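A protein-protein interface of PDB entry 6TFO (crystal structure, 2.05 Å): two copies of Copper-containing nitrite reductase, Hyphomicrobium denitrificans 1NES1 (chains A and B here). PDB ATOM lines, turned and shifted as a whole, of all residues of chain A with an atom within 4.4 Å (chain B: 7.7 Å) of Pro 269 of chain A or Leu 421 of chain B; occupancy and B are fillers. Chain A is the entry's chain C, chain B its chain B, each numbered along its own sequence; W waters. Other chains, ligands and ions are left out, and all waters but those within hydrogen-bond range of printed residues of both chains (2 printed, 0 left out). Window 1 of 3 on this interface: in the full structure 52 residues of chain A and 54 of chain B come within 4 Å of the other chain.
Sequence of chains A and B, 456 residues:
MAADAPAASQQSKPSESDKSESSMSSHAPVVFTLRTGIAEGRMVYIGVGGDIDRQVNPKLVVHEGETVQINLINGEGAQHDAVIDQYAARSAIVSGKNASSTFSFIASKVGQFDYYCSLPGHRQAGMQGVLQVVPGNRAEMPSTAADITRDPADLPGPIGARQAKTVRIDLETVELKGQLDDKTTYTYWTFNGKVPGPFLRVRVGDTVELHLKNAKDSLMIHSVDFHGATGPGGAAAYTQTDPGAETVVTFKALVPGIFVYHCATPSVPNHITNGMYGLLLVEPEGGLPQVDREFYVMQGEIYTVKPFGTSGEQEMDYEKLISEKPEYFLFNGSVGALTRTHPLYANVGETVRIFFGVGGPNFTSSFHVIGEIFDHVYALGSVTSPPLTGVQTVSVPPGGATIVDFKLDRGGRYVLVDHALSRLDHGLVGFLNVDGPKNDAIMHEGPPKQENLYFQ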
ATOM      1  N   SER A 267      16.295  -9.227 -23.498  1.00  0.00           N
ATOM      2  CA  SER A 267      15.099  -8.399 -23.551  1.00  0.00           C
ATOM      3  C   SER A 267      15.170  -7.378 -22.420  1.00  0.00           C
ATOM      4  O   SER A 267      15.258  -7.779 -21.225  1.00  0.00           O
ATOM      5  CB  SER A 267      13.846  -9.248 -23.431  1.00  0.00           C
ATOM      6  OG  SER A 267      12.659  -8.473 -23.337  1.00  0.00           O
ATOM      7  N   VAL A 268      15.124  -6.106 -22.780  1.00  0.00           N
ATOM      8  CA  VAL A 268      15.221  -5.002 -21.787  1.00  0.00           C
ATOM      9  C   VAL A 268      14.030  -5.120 -20.841  1.00  0.00           C
ATOM     10  O   VAL A 268      14.214  -5.120 -19.624  1.00  0.00           O
ATOM     11  CB  VAL A 268      15.342  -3.639 -22.493  1.00  0.00           C
ATOM     12  CG1 VAL A 268      15.394  -2.492 -21.501  1.00  0.00           C
ATOM     13  CG2 VAL A 268      16.551  -3.603 -23.410  1.00  0.00           C
ATOM     14  N   PRO A 269      12.789  -5.302 -21.351  1.00  0.00           N
ATOM     15  CA  PRO A 269      11.627  -5.486 -20.477  1.00  0.00           C
ATOM     16  C   PRO A 269      11.847  -6.604 -19.443  1.00  0.00           C
ATOM     17  O   PRO A 269      11.399  -6.459 -18.328  1.00  0.00           O
ATOM     18  CB  PRO A 269      10.496  -5.878 -21.430  1.00  0.00           C
ATOM     19  CG  PRO A 269      10.927  -5.345 -22.786  1.00  0.00           C
ATOM     20  CD  PRO A 269      12.441  -5.377 -22.781  1.00  0.00           C
ATOM     21  N   ASN A 270      12.538  -7.683 -19.843  1.00  0.00           N
ATOM     22  CA  ASN A 270      12.833  -8.863 -18.986  1.00  0.00           C
ATOM     23  C   ASN A 270      13.798  -8.435 -17.880  1.00  0.00           C
ATOM     24  O   ASN A 270      13.498  -8.674 -16.694  1.00  0.00           O
ATOM     25  CB  ASN A 270      13.390 -10.032 -19.810  1.00  0.00           C
ATOM     26  CG  ASN A 270      13.559 -11.321 -19.028  1.00  0.00           C
ATOM     27  OD1 ASN A 270      13.144 -11.425 -17.870  1.00  0.00           O
ATOM     28  ND2 ASN A 270      14.164 -12.313 -19.664  1.00  0.00           N
ATOM     29  N   HIS A 271      14.918  -7.824 -18.260  1.00  0.00           N
ATOM     30  CA  HIS A 271      15.940  -7.298 -17.314  1.00  0.00           C
ATOM     31  C   HIS A 271      15.281  -6.314 -16.337  1.00  0.00           C
ATOM     32  O   HIS A 271      15.601  -6.357 -15.147  1.00  0.00           O
ATOM     33  CB  HIS A 271      17.106  -6.698 -18.101  1.00  0.00           C
ATOM     34  CG  HIS A 271      17.929  -7.738 -18.775  1.00  0.00           C
ATOM     35  ND1 HIS A 271      19.129  -8.167 -18.256  1.00  0.00           N
ATOM     36  CD2 HIS A 271      17.728  -8.443 -19.904  1.00  0.00           C
ATOM     37  CE1 HIS A 271      19.633  -9.101 -19.039  1.00  0.00           C
ATOM     38  NE2 HIS A 271      18.798  -9.274 -20.061  1.00  0.00           N
ATOM     39  N   ILE A 272      14.338  -5.503 -16.810  1.00  0.00           N
ATOM     40  CA  ILE A 272      13.663  -4.492 -15.948  1.00  0.00           C
ATOM     41  C   ILE A 272      12.714  -5.194 -14.970  1.00  0.00           C
ATOM     42  O   ILE A 272      12.923  -5.000 -13.751  1.00  0.00           O
ATOM     43  CB  ILE A 272      13.006  -3.380 -16.783  1.00  0.00           C
ATOM     44  CG1 ILE A 272      14.076  -2.487 -17.422  1.00  0.00           C
ATOM     45  CG2 ILE A 272      12.028  -2.567 -15.941  1.00  0.00           C
ATOM     46  CD1 ILE A 272      13.532  -1.557 -18.485  1.00  0.00           C
ATOM     47  N   THR A 273      11.759  -6.013 -15.438  1.00  0.00           N
ATOM     48  CA  THR A 273      10.793  -6.723 -14.542  1.00  0.00           C
ATOM     49  C   THR A 273      11.546  -7.492 -13.448  1.00  0.00           C
ATOM     50  O   THR A 273      11.039  -7.552 -12.301  1.00  0.00           O
ATOM     51  CB  THR A 273       9.818  -7.648 -15.292  1.00  0.00           C
ATOM     52  OG1 THR A 273       8.935  -8.201 -14.314  1.00  0.00           O
ATOM     53  CG2 THR A 273      10.482  -8.771 -16.053  1.00  0.00           C
ATOM     54  N   LEU A 321       4.349 -10.994 -19.864  1.00  0.00           N
ATOM     55  CA  LEU A 321       5.286  -9.849 -19.976  1.00  0.00           C
ATOM     56  C   LEU A 321       4.988  -9.066 -21.263  1.00  0.00           C
ATOM     57  O   LEU A 321       4.715  -7.867 -21.149  1.00  0.00           O
ATOM     58  CB  LEU A 321       6.734 -10.351 -19.928  1.00  0.00           C
ATOM     59  CG  LEU A 321       7.804  -9.272 -20.078  1.00  0.00           C
ATOM     60  CD1 LEU A 321       7.690  -8.223 -18.989  1.00  0.00           C
ATOM     61  CD2 LEU A 321       9.191  -9.883 -20.084  1.00  0.00           C
ATOM     62  N   PRO A 361       8.334  -2.738 -16.090  1.00  0.00           N
ATOM     63  CA  PRO A 361       8.599  -1.993 -17.322  1.00  0.00           C
ATOM     64  C   PRO A 361       7.437  -1.325 -18.071  1.00  0.00           C
ATOM     65  O   PRO A 361       7.727  -0.662 -19.042  1.00  0.00           O
ATOM     66  CB  PRO A 361       9.100  -3.095 -18.266  1.00  0.00           C
ATOM     67  CG  PRO A 361       8.330  -4.305 -17.834  1.00  0.00           C
ATOM     68  CD  PRO A 361       8.343  -4.190 -16.322  1.00  0.00           C
ATOM     69  N   ASN A 362       6.179  -1.504 -17.655  1.00  0.00           N
ATOM     70  CA  ASN A 362       5.048  -1.214 -18.576  1.00  0.00           C
ATOM     71  C   ASN A 362       4.036  -0.205 -18.027  1.00  0.00           C
ATOM     72  O   ASN A 362       3.508   0.525 -18.874  1.00  0.00           O
ATOM     73  CB  ASN A 362       4.374  -2.512 -18.994  1.00  0.00           C
ATOM     74  CG  ASN A 362       5.267  -3.288 -19.932  1.00  0.00           C
ATOM     75  OD1 ASN A 362       5.808  -2.720 -20.865  1.00  0.00           O
ATOM     76  ND2 ASN A 362       5.415  -4.577 -19.697  1.00  0.00           N
ATOM     77  N   GLN B  69      18.063 -12.568 -29.863  1.00  0.00           N
ATOM     78  CA  GLN B  69      17.225 -12.824 -28.670  1.00  0.00           C
ATOM     79  C   GLN B  69      16.481 -14.145 -28.909  1.00  0.00           C
ATOM     80  O   GLN B  69      15.787 -14.274 -29.951  1.00  0.00           O
ATOM     81  CB  GLN B  69      16.252 -11.667 -28.453  1.00  0.00           C
ATOM     82  CG  GLN B  69      15.438 -11.815 -27.176  1.00  0.00           C
ATOM     83  CD  GLN B  69      14.478 -10.672 -26.967  1.00  0.00           C
ATOM     84  OE1 GLN B  69      14.812  -9.507 -27.196  1.00  0.00           O
ATOM     85  NE2 GLN B  69      13.276 -11.000 -26.504  1.00  0.00           N
ATOM     86  N   THR B 102      14.350 -15.652 -21.439  1.00  0.00           N
ATOM     87  CA  THR B 102      14.948 -15.081 -22.665  1.00  0.00           C
ATOM     88  C   THR B 102      16.422 -14.832 -22.369  1.00  0.00           C
ATOM     89  O   THR B 102      16.774 -14.656 -21.178  1.00  0.00           O
ATOM     90  CB  THR B 102      14.137 -13.893 -23.194  1.00  0.00           C
ATOM     91  OG1 THR B 102      14.629 -12.736 -22.530  1.00  0.00           O
ATOM     92  CG2 THR B 102      12.646 -14.079 -23.011  1.00  0.00           C
ATOM     93  N   SER B 366       4.838   6.648 -23.104  1.00  0.00           N
ATOM     94  CA  SER B 366       5.890   7.168 -22.213  1.00  0.00           C
ATOM     95  C   SER B 366       7.097   7.531 -23.095  1.00  0.00           C
ATOM     96  O   SER B 366       8.101   6.790 -23.086  1.00  0.00           O
ATOM     97  CB  SER B 366       6.187   6.170 -21.132  1.00  0.00           C
ATOM     98  OG  SER B 366       4.998   5.926 -20.389  1.00  0.00           O
ATOM     99  N   HIS B 368      10.314   8.781 -24.956  1.00  0.00           N
ATOM    100  CA  HIS B 368      11.700   8.866 -24.450  1.00  0.00           C
ATOM    101  C   HIS B 368      12.660   8.622 -25.604  1.00  0.00           C
ATOM    102  O   HIS B 368      12.311   7.853 -26.510  1.00  0.00           O
ATOM    103  CB  HIS B 368      11.913   7.857 -23.321  1.00  0.00           C
ATOM    104  CG  HIS B 368      13.337   7.708 -22.894  1.00  0.00           C
ATOM    105  ND1 HIS B 368      13.906   8.528 -21.938  1.00  0.00           N
ATOM    106  CD2 HIS B 368      14.294   6.828 -23.259  1.00  0.00           C
ATOM    107  CE1 HIS B 368      15.153   8.166 -21.735  1.00  0.00           C
ATOM    108  NE2 HIS B 368      15.416   7.122 -22.534  1.00  0.00           N
ATOM    109  N   ILE B 370      16.430   7.296 -26.051  1.00  0.00           N
ATOM    110  CA  ILE B 370      17.560   6.642 -25.341  1.00  0.00           C
ATOM    111  C   ILE B 370      18.831   7.391 -25.746  1.00  0.00           C
ATOM    112  O   ILE B 370      19.029   7.601 -26.959  1.00  0.00           O
ATOM    113  CB  ILE B 370      17.619   5.127 -25.652  1.00  0.00           C
ATOM    114  CG1 ILE B 370      16.268   4.446 -25.379  1.00  0.00           C
ATOM    115  CG2 ILE B 370      18.765   4.458 -24.894  1.00  0.00           C
ATOM    116  CD1 ILE B 370      16.267   2.935 -25.525  1.00  0.00           C
ATOM    117  N   LEU B 416      14.231   6.296 -30.269  1.00  0.00           N
ATOM    118  CA  LEU B 416      12.859   6.687 -29.850  1.00  0.00           C
ATOM    119  C   LEU B 416      12.098   5.443 -29.354  1.00  0.00           C
ATOM    120  O   LEU B 416      12.055   4.427 -30.103  1.00  0.00           O
ATOM    121  CB  LEU B 416      12.131   7.282 -31.058  1.00  0.00           C
ATOM    122  CG  LEU B 416      12.516   8.689 -31.503  1.00  0.00           C
ATOM    123  CD1 LEU B 416      13.913   8.714 -32.102  1.00  0.00           C
ATOM    124  CD2 LEU B 416      11.506   9.203 -32.512  1.00  0.00           C
ATOM    125  N   VAL B 417      11.502   5.510 -28.161  1.00  0.00           N
ATOM    126  CA  VAL B 417      10.722   4.388 -27.553  1.00  0.00           C
ATOM    127  C   VAL B 417       9.500   4.948 -26.818  1.00  0.00           C
ATOM    128  O   VAL B 417       9.516   6.122 -26.398  1.00  0.00           O
ATOM    129  CB  VAL B 417      11.577   3.559 -26.573  1.00  0.00           C
ATOM    130  CG1 VAL B 417      12.827   3.011 -27.232  1.00  0.00           C
ATOM    131  CG2 VAL B 417      11.933   4.327 -25.305  1.00  0.00           C
ATOM    132  N   ASP B 418       8.482   4.113 -26.657  1.00  0.00           N
ATOM    133  CA  ASP B 418       7.489   4.198 -25.561  1.00  0.00           C
ATOM    134  C   ASP B 418       8.116   3.401 -24.420  1.00  0.00           C
ATOM    135  O   ASP B 418       8.486   2.295 -24.650  1.00  0.00           O
ATOM    136  CB  ASP B 418       6.137   3.693 -26.047  1.00  0.00           C
ATOM    137  CG  ASP B 418       5.004   3.770 -25.047  1.00  0.00           C
ATOM    138  OD1 ASP B 418       5.286   3.878 -23.830  1.00  0.00           O
ATOM    139  OD2 ASP B 418       3.840   3.716 -25.511  1.00  0.00           O
ATOM    140  N   HIS B 419       8.337   3.995 -23.261  1.00  0.00           N
ATOM    141  CA  HIS B 419       9.138   3.369 -22.180  1.00  0.00           C
ATOM    142  C   HIS B 419       8.292   2.342 -21.425  1.00  0.00           C
ATOM    143  O   HIS B 419       8.799   1.825 -20.389  1.00  0.00           O
ATOM    144  CB  HIS B 419       9.756   4.415 -21.243  1.00  0.00           C
ATOM    145  CG  HIS B 419      11.126   4.035 -20.798  1.00  0.00           C
ATOM    146  ND1 HIS B 419      11.333   3.067 -19.866  1.00  0.00           N
ATOM    147  CD2 HIS B 419      12.347   4.488 -21.158  1.00  0.00           C
ATOM    148  CE1 HIS B 419      12.627   2.942 -19.641  1.00  0.00           C
ATOM    149  NE2 HIS B 419      13.268   3.805 -20.410  1.00  0.00           N
ATOM    150  N   ALA B 420       7.054   2.086 -21.882  1.00  0.00           N
ATOM    151  CA  ALA B 420       6.335   0.823 -21.592  1.00  0.00           C
ATOM    152  C   ALA B 420       6.945  -0.226 -22.519  1.00  0.00           C
ATOM    153  O   ALA B 420       6.415  -0.429 -23.621  1.00  0.00           O
ATOM    154  CB  ALA B 420       4.845   0.969 -21.784  1.00  0.00           C
ATOM    155  N   LEU B 421       8.087  -0.794 -22.118  1.00  0.00           N
ATOM    156  CA  LEU B 421       9.109  -1.286 -23.070  1.00  0.00           C
ATOM    157  C   LEU B 421       8.754  -2.663 -23.631  1.00  0.00           C
ATOM    158  O   LEU B 421       9.460  -3.090 -24.604  1.00  0.00           O
ATOM    159  CB  LEU B 421      10.471  -1.297 -22.372  1.00  0.00           C
ATOM    160  CG  LEU B 421      11.201   0.055 -22.355  1.00  0.00           C
ATOM    161  CD1 LEU B 421      12.528  -0.082 -21.627  1.00  0.00           C
ATOM    162  CD2 LEU B 421      11.444   0.594 -23.762  1.00  0.00           C
ATOM    163  N   SER B 422       7.717  -3.325 -23.101  1.00  0.00           N
ATOM    164  CA  SER B 422       7.194  -4.553 -23.748  1.00  0.00           C
ATOM    165  C   SER B 422       6.755  -4.188 -25.181  1.00  0.00           C
ATOM    166  O   SER B 422       6.732  -5.066 -26.044  1.00  0.00           O
ATOM    167  CB  SER B 422       6.127  -5.199 -22.935  1.00  0.00           C
ATOM    168  OG  SER B 422       6.701  -5.876 -21.828  1.00  0.00           O
ATOM    169  N   ARG B 423       6.497  -2.912 -25.459  1.00  0.00           N
ATOM    170  CA  ARG B 423       6.015  -2.481 -26.793  1.00  0.00           C
ATOM    171  C   ARG B 423       7.168  -2.499 -27.800  1.00  0.00           C
ATOM    172  O   ARG B 423       6.870  -2.472 -28.990  1.00  0.00           O
ATOM    173  CB  ARG B 423       5.310  -1.141 -26.670  1.00  0.00           C
ATOM    174  CG  ARG B 423       4.089  -1.249 -25.779  1.00  0.00           C
ATOM    175  CD  ARG B 423       3.439   0.073 -25.466  1.00  0.00           C
ATOM    176  NE  ARG B 423       2.594  -0.088 -24.297  1.00  0.00           N
ATOM    177  CZ  ARG B 423       1.905   0.874 -23.695  1.00  0.00           C
ATOM    178  NH1 ARG B 423       1.951   2.115 -24.148  1.00  0.00           N
ATOM    179  NH2 ARG B 423       1.172   0.594 -22.626  1.00  0.00           N
ATOM    180  N   LEU B 424       8.421  -2.613 -27.356  1.00  0.00           N
ATOM    181  CA  LEU B 424       9.559  -2.969 -28.246  1.00  0.00           C
ATOM    182  C   LEU B 424       9.209  -4.261 -28.999  1.00  0.00           C
ATOM    183  O   LEU B 424       9.419  -4.337 -30.229  1.00  0.00           O
ATOM    184  CB  LEU B 424      10.814  -3.215 -27.410  1.00  0.00           C
ATOM    185  CG  LEU B 424      11.547  -2.003 -26.869  1.00  0.00           C
ATOM    186  CD1 LEU B 424      12.686  -2.472 -25.979  1.00  0.00           C
ATOM    187  CD2 LEU B 424      12.068  -1.130 -28.001  1.00  0.00           C
ATOM    188  N   ASP B 425       8.701  -5.256 -28.266  1.00  0.00           N
ATOM    189  CA  ASP B 425       8.425  -6.618 -28.787  1.00  0.00           C
ATOM    190  C   ASP B 425       7.134  -6.599 -29.624  1.00  0.00           C
ATOM    191  O   ASP B 425       6.737  -7.669 -30.057  1.00  0.00           O
ATOM    192  CB  ASP B 425       8.419  -7.624 -27.636  1.00  0.00           C
ATOM    193  CG  ASP B 425       9.682  -7.592 -26.775  1.00  0.00           C
ATOM    194  OD1 ASP B 425      10.774  -7.644 -27.337  1.00  0.00           O
ATOM    195  OD2 ASP B 425       9.570  -7.533 -25.538  1.00  0.00           O
ATOM    196  N   HIS B 426       6.531  -5.438 -29.909  1.00  0.00           N
ATOM    197  CA  HIS B 426       5.349  -5.287 -30.815  1.00  0.00           C
ATOM    198  C   HIS B 426       5.608  -4.285 -31.954  1.00  0.00           C
ATOM    199  O   HIS B 426       4.606  -3.850 -32.578  1.00  0.00           O
ATOM    200  CB  HIS B 426       4.090  -4.867 -30.028  1.00  0.00           C
ATOM    201  CG  HIS B 426       3.586  -5.902 -29.073  1.00  0.00           C
ATOM    202  ND1 HIS B 426       2.626  -6.835 -29.424  1.00  0.00           N
ATOM    203  CD2 HIS B 426       3.893  -6.137 -27.781  1.00  0.00           C
ATOM    204  CE1 HIS B 426       2.376  -7.609 -28.392  1.00  0.00           C
ATOM    205  NE2 HIS B 426       3.135  -7.202 -27.372  1.00  0.00           N
ATOM    206  N   LEU B 428       7.530  -1.222 -31.812  1.00  0.00           N
ATOM    207  CA  LEU B 428       7.620   0.215 -31.424  1.00  0.00           C
ATOM    208  C   LEU B 428       9.058   0.598 -31.075  1.00  0.00           C
ATOM    209  O   LEU B 428       9.441   0.504 -29.885  1.00  0.00           O
ATOM    210  CB  LEU B 428       6.695   0.514 -30.240  1.00  0.00           C
ATOM    211  CG  LEU B 428       6.443   2.000 -29.989  1.00  0.00           C
ATOM    212  CD1 LEU B 428       5.866   2.663 -31.240  1.00  0.00           C
ATOM    213  CD2 LEU B 428       5.502   2.178 -28.816  1.00  0.00           C
HETATM  214  O   HOH W   1      10.411   0.798 -18.332  1.00  0.00           O
HETATM  215  O   HOH W   2      16.514 -11.271 -21.467  1.00  0.00           O
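The side-chain hydroxyl (OG1) of Thr 102 of chain B is in hydrogen-bond range of the side-chain amide nitrogen (ND2) of Asn 270 of chain A.
O of Pro 361 of chain A lies within hydrogen-bond range of N of Leu 421 of chain B.
The backbone NH (N) of Leu 421 of chain B sits at hydrogen-bond distance from the side-chain amide oxygen (OD1) of Asn 362 of chain A, at 3.2 Å.
The side-chain hydroxyl (OG) of Ser 422 of chain B sits at hydrogen-bond distance from the backbone carbonyl oxygen (O) of Leu 321 of chain A (2.9 Å).
OG of Ser 422 of chain B lies within hydrogen-bond range of ND2 of Asn 362 of chain A (2.8 Å).
O of Pro 361 of chain A sits close to O of His 419 of chain B (3.0 Å).
The backbone NH of His 419 of chain B sits at hydrogen-bond distance from the backbone carbonyl oxygen of Ser 366 of chain B, at 2.8 Å.
The side-chain carboxylate (OD1) of Asp 418 of chain B sits close to the backbone NH (N) of Ala 420 of chain B, 3.2 Å away.
Gln 69 of chain B touches Ser 267 of chain A.
Ser 267 of chain A touches Thr 102 of chain B.
OD2 of Asp 425 of chain B touches OG of Ser 267 of chain A (3.9 Å).
Leu 421 of chain B touches Val 268 of chain A (CD1 to CG1, 3.7 Å).
Pro 269 of chain A touches Leu 421 of chain B.
Pro 269 of chain A touches Ser 422 of chain B.
Pro 269 of chain A touches Asp 425 of chain B (CG to OD2, 3.8 Å).
CD1 of Leu 421 of chain B touches CD1 of Ile 272 of chain A (3.6 Å).
Ala 420 of chain B touches Pro 361 of chain A.
Asn 362 of chain A touches Ala 420 of chain B (OD1 to C, 3.2 Å).
Of the printed residues of chain B, Ser 267 of chain A touches Gln 69 (3.6 Å), Thr 102 (3.7 Å) and Asp 425 (3.9 Å).
Of the printed residues of chain B, Val 268 of chain A touches Leu 421 (3.7 Å).
Of chain B, only Leu 421, Ser 422 and Asp 425 come within 4 Å of Pro 269 of chain A.
Printed residues of chain B within 4 Å of Asn 270 of chain A: Thr 102.
Thr 273 of chain A touches none of the printed residues of chain B.
Printed residues of chain A within 4 Å of Gln 69 of chain B: Ser 267.
Ile 370 of chain B touches none of the printed residues of chain A.
Of chain A, only Val 268 (3.7 Å), Pro 269 (3.2 Å), Ile 272 (3.6 Å), Pro 361 (3.1 Å) and Asn 362 (3.2 Å) come within 4 Å of Leu 421 of chain B.
Of the printed residues of chain A, Asp 425 of chain B touches Ser 267 (3.9 Å) and Pro 269 (3.8 Å).
The nearest printed residue of chain A that does not touch Leu 421 of chain B is Ser 267 of chain A (6.4 Å).
Of the 10 printed residues of chain A, 8 touch a printed residue of chain B.
No position is printed for both chains.
Of the 16 pairs that touch across the chains among the printed residues, none has its exchanged pair printed and touching as well.
Water W2 lies within hydrogen-bond range of OG1 of Thr 102 of chain B, N of Ser 267 of chain A, ND2 of Asn 270 of chain A and NE2 of His 271 of chain A.
Water W1 lies within hydrogen-bond range of O of His 419 of chain B and O of Pro 361 of chain A.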
